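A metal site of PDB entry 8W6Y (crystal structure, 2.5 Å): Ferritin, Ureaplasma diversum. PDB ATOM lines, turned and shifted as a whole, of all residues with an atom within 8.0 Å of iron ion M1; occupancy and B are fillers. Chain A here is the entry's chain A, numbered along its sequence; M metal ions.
The side-chain carboxylate of Asp 138 is in salt-bridge range of the side-chain amino group of Lys 141. The side-chain amino group of Lys 141 is in salt-bridge range of the side-chain carboxylate of Asp 142 (2.8 Å). NZ of Lys 61 sits close to OD2 of Asp 142, at 3.2 Å. OD1 of Asn 27 sits at hydrogen-bond distance from ND1 of His 65, 3.3 Å away. The backbone carbonyl oxygen (O) of His 65 sits at hydrogen-bond distance from the side-chain hydroxyl (OH) of Tyr 135 (2.7 Å).
Iron ion M1 is bound by OD2 of Asp 138 (1.9 Å), OD2 of Asp 142 (2.1 Å), OD2 of Asp 60 (2.1 Å) and NE2 of His 65 (2.3 Å).
Merely in contact with iron ion M1: Lys 141 (3.4 Å).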
ATOM      1  N   ASN A  27      23.326  28.577  18.515  1.00  0.00           N
ATOM      2  CA  ASN A  27      23.033  28.307  19.915  1.00  0.00           C
ATOM      3  C   ASN A  27      23.445  29.472  20.796  1.00  0.00           C
ATOM      4  O   ASN A  27      22.734  29.822  21.745  1.00  0.00           O
ATOM      5  CB  ASN A  27      23.692  26.995  20.377  1.00  0.00           C
ATOM      6  CG  ASN A  27      22.854  25.776  20.006  1.00  0.00           C
ATOM      7  OD1 ASN A  27      21.796  25.527  20.595  1.00  0.00           O
ATOM      8  ND2 ASN A  27      23.288  25.033  18.991  1.00  0.00           N
ATOM      9  N   HIS A  56      16.569  28.534  31.975  1.00  0.00           N
ATOM     10  CA  HIS A  56      17.205  27.225  31.889  1.00  0.00           C
ATOM     11  C   HIS A  56      17.438  26.809  30.439  1.00  0.00           C
ATOM     12  O   HIS A  56      18.452  26.166  30.136  1.00  0.00           O
ATOM     13  CB  HIS A  56      16.364  26.177  32.628  1.00  0.00           C
ATOM     14  CG  HIS A  56      16.609  26.140  34.113  1.00  0.00           C
ATOM     15  ND1 HIS A  56      17.073  25.013  34.770  1.00  0.00           N
ATOM     16  CD2 HIS A  56      16.436  27.077  35.075  1.00  0.00           C
ATOM     17  CE1 HIS A  56      17.191  25.276  36.065  1.00  0.00           C
ATOM     18  NE2 HIS A  56      16.811  26.516  36.268  1.00  0.00           N
ATOM     19  N   LEU A  57      16.528  27.162  29.533  1.00  0.00           N
ATOM     20  CA  LEU A  57      16.730  26.892  28.117  1.00  0.00           C
ATOM     21  C   LEU A  57      17.853  27.760  27.562  1.00  0.00           C
ATOM     22  O   LEU A  57      18.665  27.297  26.735  1.00  0.00           O
ATOM     23  CB  LEU A  57      15.422  27.115  27.357  1.00  0.00           C
ATOM     24  CG  LEU A  57      15.236  26.579  25.933  1.00  0.00           C
ATOM     25  CD1 LEU A  57      15.531  25.100  25.837  1.00  0.00           C
ATOM     26  CD2 LEU A  57      13.810  26.866  25.472  1.00  0.00           C
ATOM     27  N   GLU A  59      20.510  28.787  29.312  1.00  0.00           N
ATOM     28  CA  GLU A  59      21.769  28.218  29.789  1.00  0.00           C
ATOM     29  C   GLU A  59      22.106  26.906  29.086  1.00  0.00           C
ATOM     30  O   GLU A  59      23.284  26.597  28.881  1.00  0.00           O
ATOM     31  CB  GLU A  59      21.707  28.038  31.304  1.00  0.00           C
ATOM     32  CG  GLU A  59      21.829  29.378  31.991  1.00  0.00           C
ATOM     33  CD  GLU A  59      21.255  29.396  33.393  1.00  0.00           C
ATOM     34  OE1 GLU A  59      21.322  30.480  34.010  1.00  0.00           O
ATOM     35  OE2 GLU A  59      20.754  28.339  33.866  1.00  0.00           O
ATOM     36  N   ASP A  60      21.090  26.127  28.733  1.00  0.00           N
ATOM     37  CA  ASP A  60      21.263  24.948  27.896  1.00  0.00           C
ATOM     38  C   ASP A  60      21.940  25.293  26.568  1.00  0.00           C
ATOM     39  O   ASP A  60      22.963  24.698  26.203  1.00  0.00           O
ATOM     40  CB  ASP A  60      19.895  24.305  27.701  1.00  0.00           C
ATOM     41  CG  ASP A  60      19.967  22.942  27.084  1.00  0.00           C
ATOM     42  OD1 ASP A  60      20.961  22.223  27.334  1.00  0.00           O
ATOM     43  OD2 ASP A  60      19.004  22.625  26.350  1.00  0.00           O
ATOM     44  N   LYS A  61      21.390  26.274  25.819  1.00  0.00           N
ATOM     45  CA  LYS A  61      21.949  26.644  24.516  1.00  0.00           C
ATOM     46  C   LYS A  61      23.345  27.242  24.648  1.00  0.00           C
ATOM     47  O   LYS A  61      24.224  26.993  23.814  1.00  0.00           O
ATOM     48  CB  LYS A  61      21.045  27.642  23.769  1.00  0.00           C
ATOM     49  CG  LYS A  61      19.569  27.256  23.548  1.00  0.00           C
ATOM     50  CD  LYS A  61      19.405  26.022  22.656  1.00  0.00           C
ATOM     51  CE  LYS A  61      17.936  25.756  22.315  1.00  0.00           C
ATOM     52  NZ  LYS A  61      17.732  24.367  21.786  1.00  0.00           N
ATOM     53  N   VAL A  64      26.020  23.390  27.066  1.00  0.00           N
ATOM     54  CA  VAL A  64      26.425  22.131  26.462  1.00  0.00           C
ATOM     55  C   VAL A  64      26.176  22.137  24.952  1.00  0.00           C
ATOM     56  O   VAL A  64      26.881  21.452  24.199  1.00  0.00           O
ATOM     57  CB  VAL A  64      25.714  20.944  27.140  1.00  0.00           C
ATOM     58  CG1 VAL A  64      26.118  20.868  28.609  1.00  0.00           C
ATOM     59  CG2 VAL A  64      24.175  21.027  26.974  1.00  0.00           C
ATOM     60  N   HIS A  65      25.182  22.905  24.480  1.00  0.00           N
ATOM     61  CA  HIS A  65      24.903  22.931  23.048  1.00  0.00           C
ATOM     62  C   HIS A  65      26.088  23.503  22.286  1.00  0.00           C
ATOM     63  O   HIS A  65      26.406  23.042  21.183  1.00  0.00           O
ATOM     64  CB  HIS A  65      23.631  23.727  22.759  1.00  0.00           C
ATOM     65  CG  HIS A  65      22.368  22.944  22.945  1.00  0.00           C
ATOM     66  ND1 HIS A  65      21.638  22.461  21.870  1.00  0.00           N
ATOM     67  CD2 HIS A  65      21.691  22.578  24.057  1.00  0.00           C
ATOM     68  CE1 HIS A  65      20.565  21.831  22.327  1.00  0.00           C
ATOM     69  NE2 HIS A  65      20.575  21.883  23.650  1.00  0.00           N
ATOM     70  N   GLU A 106      12.753  26.652  18.274  1.00  0.00           N
ATOM     71  CA  GLU A 106      13.149  25.258  18.519  1.00  0.00           C
ATOM     72  C   GLU A 106      12.757  24.349  17.362  1.00  0.00           C
ATOM     73  O   GLU A 106      13.500  23.397  17.049  1.00  0.00           O
ATOM     74  CB  GLU A 106      12.529  24.740  19.811  1.00  0.00           C
ATOM     75  CG  GLU A 106      12.946  25.523  21.041  1.00  0.00           C
ATOM     76  CD  GLU A 106      14.436  25.466  21.281  1.00  0.00           C
ATOM     77  OE1 GLU A 106      14.991  24.354  21.384  1.00  0.00           O
ATOM     78  OE2 GLU A 106      15.056  26.546  21.354  1.00  0.00           O
ATOM     79  N   VAL A 109      15.475  24.720  15.023  1.00  0.00           N
ATOM     80  CA  VAL A 109      16.609  23.893  15.444  1.00  0.00           C
ATOM     81  C   VAL A 109      16.492  22.485  14.858  1.00  0.00           C
ATOM     82  O   VAL A 109      17.475  21.931  14.335  1.00  0.00           O
ATOM     83  CB  VAL A 109      16.712  23.837  16.982  1.00  0.00           C
ATOM     84  CG1 VAL A 109      17.675  22.705  17.399  1.00  0.00           C
ATOM     85  CG2 VAL A 109      17.193  25.204  17.531  1.00  0.00           C
ATOM     86  N   TRP A 134      23.030  13.129  19.229  1.00  0.00           N
ATOM     87  CA  TRP A 134      22.601  13.820  20.438  1.00  0.00           C
ATOM     88  C   TRP A 134      21.723  15.028  20.102  1.00  0.00           C
ATOM     89  O   TRP A 134      20.651  15.214  20.682  1.00  0.00           O
ATOM     90  CB  TRP A 134      23.805  14.255  21.283  1.00  0.00           C
ATOM     91  CG  TRP A 134      23.357  14.860  22.586  1.00  0.00           C
ATOM     92  CD1 TRP A 134      23.060  14.184  23.737  1.00  0.00           C
ATOM     93  CD2 TRP A 134      23.092  16.260  22.856  1.00  0.00           C
ATOM     94  NE1 TRP A 134      22.648  15.070  24.714  1.00  0.00           N
ATOM     95  CE2 TRP A 134      22.650  16.340  24.203  1.00  0.00           C
ATOM     96  CE3 TRP A 134      23.169  17.427  22.104  1.00  0.00           C
ATOM     97  CZ2 TRP A 134      22.305  17.563  24.808  1.00  0.00           C
ATOM     98  CZ3 TRP A 134      22.823  18.650  22.709  1.00  0.00           C
ATOM     99  CH2 TRP A 134      22.406  18.694  24.047  1.00  0.00           C
ATOM    100  N   TYR A 135      22.176  15.840  19.154  1.00  0.00           N
ATOM    101  CA  TYR A 135      21.379  16.989  18.746  1.00  0.00           C
ATOM    102  C   TYR A 135      20.087  16.564  18.068  1.00  0.00           C
ATOM    103  O   TYR A 135      19.062  17.236  18.241  1.00  0.00           O
ATOM    104  CB  TYR A 135      22.200  17.887  17.826  1.00  0.00           C
ATOM    105  CG  TYR A 135      23.344  18.563  18.526  1.00  0.00           C
ATOM    106  CD1 TYR A 135      24.547  17.901  18.710  1.00  0.00           C
ATOM    107  CD2 TYR A 135      23.214  19.858  19.014  1.00  0.00           C
ATOM    108  CE1 TYR A 135      25.612  18.523  19.365  1.00  0.00           C
ATOM    109  CE2 TYR A 135      24.266  20.498  19.665  1.00  0.00           C
ATOM    110  CZ  TYR A 135      25.467  19.820  19.836  1.00  0.00           C
ATOM    111  OH  TYR A 135      26.531  20.442  20.491  1.00  0.00           O
ATOM    112  N   ARG A 137      18.172  14.074  18.893  1.00  0.00           N
ATOM    113  CA  ARG A 137      17.231  13.801  19.943  1.00  0.00           C
ATOM    114  C   ARG A 137      16.869  15.032  20.735  1.00  0.00           C
ATOM    115  O   ARG A 137      15.729  15.230  21.088  1.00  0.00           O
ATOM    116  CB  ARG A 137      17.749  12.707  20.855  1.00  0.00           C
ATOM    117  CG  ARG A 137      16.728  12.151  21.823  1.00  0.00           C
ATOM    118  CD  ARG A 137      17.117  10.766  22.301  1.00  0.00           C
ATOM    119  NE  ARG A 137      17.480  10.739  23.717  1.00  0.00           N
ATOM    120  CZ  ARG A 137      17.518   9.645  24.467  1.00  0.00           C
ATOM    121  NH1 ARG A 137      17.224   8.465  23.938  1.00  0.00           N
ATOM    122  NH2 ARG A 137      17.871   9.717  25.745  1.00  0.00           N
ATOM    123  N   ASP A 138      17.851  15.855  21.041  1.00  0.00           N
ATOM    124  CA  ASP A 138      17.562  17.023  21.865  1.00  0.00           C
ATOM    125  C   ASP A 138      16.682  18.029  21.152  1.00  0.00           C
ATOM    126  O   ASP A 138      15.950  18.771  21.824  1.00  0.00           O
ATOM    127  CB  ASP A 138      18.843  17.698  22.344  1.00  0.00           C
ATOM    128  CG  ASP A 138      18.661  18.361  23.684  1.00  0.00           C
ATOM    129  OD1 ASP A 138      18.232  17.690  24.645  1.00  0.00           O
ATOM    130  OD2 ASP A 138      18.919  19.578  23.754  1.00  0.00           O
ATOM    131  N   GLY A 139      16.739  18.076  19.820  1.00  0.00           N
ATOM    132  CA  GLY A 139      15.828  18.947  19.090  1.00  0.00           C
ATOM    133  C   GLY A 139      14.381  18.669  19.407  1.00  0.00           C
ATOM    134  O   GLY A 139      13.586  19.592  19.605  1.00  0.00           O
ATOM    135  N   LYS A 141      13.303  16.837  22.196  1.00  0.00           N
ATOM    136  CA  LYS A 141      13.099  17.011  23.636  1.00  0.00           C
ATOM    137  C   LYS A 141      12.853  18.474  24.001  1.00  0.00           C
ATOM    138  O   LYS A 141      11.882  18.794  24.700  1.00  0.00           O
ATOM    139  CB  LYS A 141      14.320  16.464  24.399  1.00  0.00           C
ATOM    140  CG  LYS A 141      14.217  16.535  25.931  1.00  0.00           C
ATOM    141  CD  LYS A 141      15.526  17.002  26.570  1.00  0.00           C
ATOM    142  CE  LYS A 141      15.547  18.516  26.768  1.00  0.00           C
ATOM    143  NZ  LYS A 141      16.919  19.134  26.817  1.00  0.00           N
ATOM    144  N   ASP A 142      13.738  19.377  23.563  1.00  0.00           N
ATOM    145  CA  ASP A 142      13.568  20.793  23.858  1.00  0.00           C
ATOM    146  C   ASP A 142      12.254  21.308  23.283  1.00  0.00           C
ATOM    147  O   ASP A 142      11.546  22.086  23.920  1.00  0.00           O
ATOM    148  CB  ASP A 142      14.729  21.616  23.304  1.00  0.00           C
ATOM    149  CG  ASP A 142      15.991  21.548  24.186  1.00  0.00           C
ATOM    150  OD1 ASP A 142      15.864  21.272  25.398  1.00  0.00           O
ATOM    151  OD2 ASP A 142      17.101  21.799  23.647  1.00  0.00           O
ATOM    152  N   LEU A 143      11.921  20.885  22.053  1.00  0.00           N
ATOM    153  CA  LEU A 143      10.668  21.320  21.453  1.00  0.00           C
ATOM    154  C   LEU A 143       9.466  20.823  22.254  1.00  0.00           C
ATOM    155  O   LEU A 143       8.491  21.554  22.439  1.00  0.00           O
ATOM    156  CB  LEU A 143      10.572  20.832  19.998  1.00  0.00           C
ATOM    157  CG  LEU A 143       9.236  21.250  19.372  1.00  0.00           C
ATOM    158  CD1 LEU A 143       9.399  22.640  18.792  1.00  0.00           C
ATOM    159  CD2 LEU A 143       8.749  20.260  18.319  1.00  0.00           C
ATOM    160  N   GLU A 145       9.332  19.988  25.576  1.00  0.00           N
ATOM    161  CA  GLU A 145       9.248  20.746  26.824  1.00  0.00           C
ATOM    162  C   GLU A 145       8.644  22.119  26.582  1.00  0.00           C
ATOM    163  O   GLU A 145       7.783  22.559  27.352  1.00  0.00           O
ATOM    164  CB  GLU A 145      10.634  20.892  27.446  1.00  0.00           C
ATOM    165  CG  GLU A 145      11.256  19.581  27.881  1.00  0.00           C
ATOM    166  CD  GLU A 145      12.631  19.769  28.483  1.00  0.00           C
ATOM    167  OE1 GLU A 145      13.172  20.903  28.424  1.00  0.00           O
ATOM    168  OE2 GLU A 145      13.179  18.760  28.993  1.00  0.00           O
HETATM  169 FE    FE M   1      18.757  21.176  24.806  1.00  0.00          FE
HETATM  170 FE    FE M   2      17.284  20.578  30.671  1.00  0.00          FE
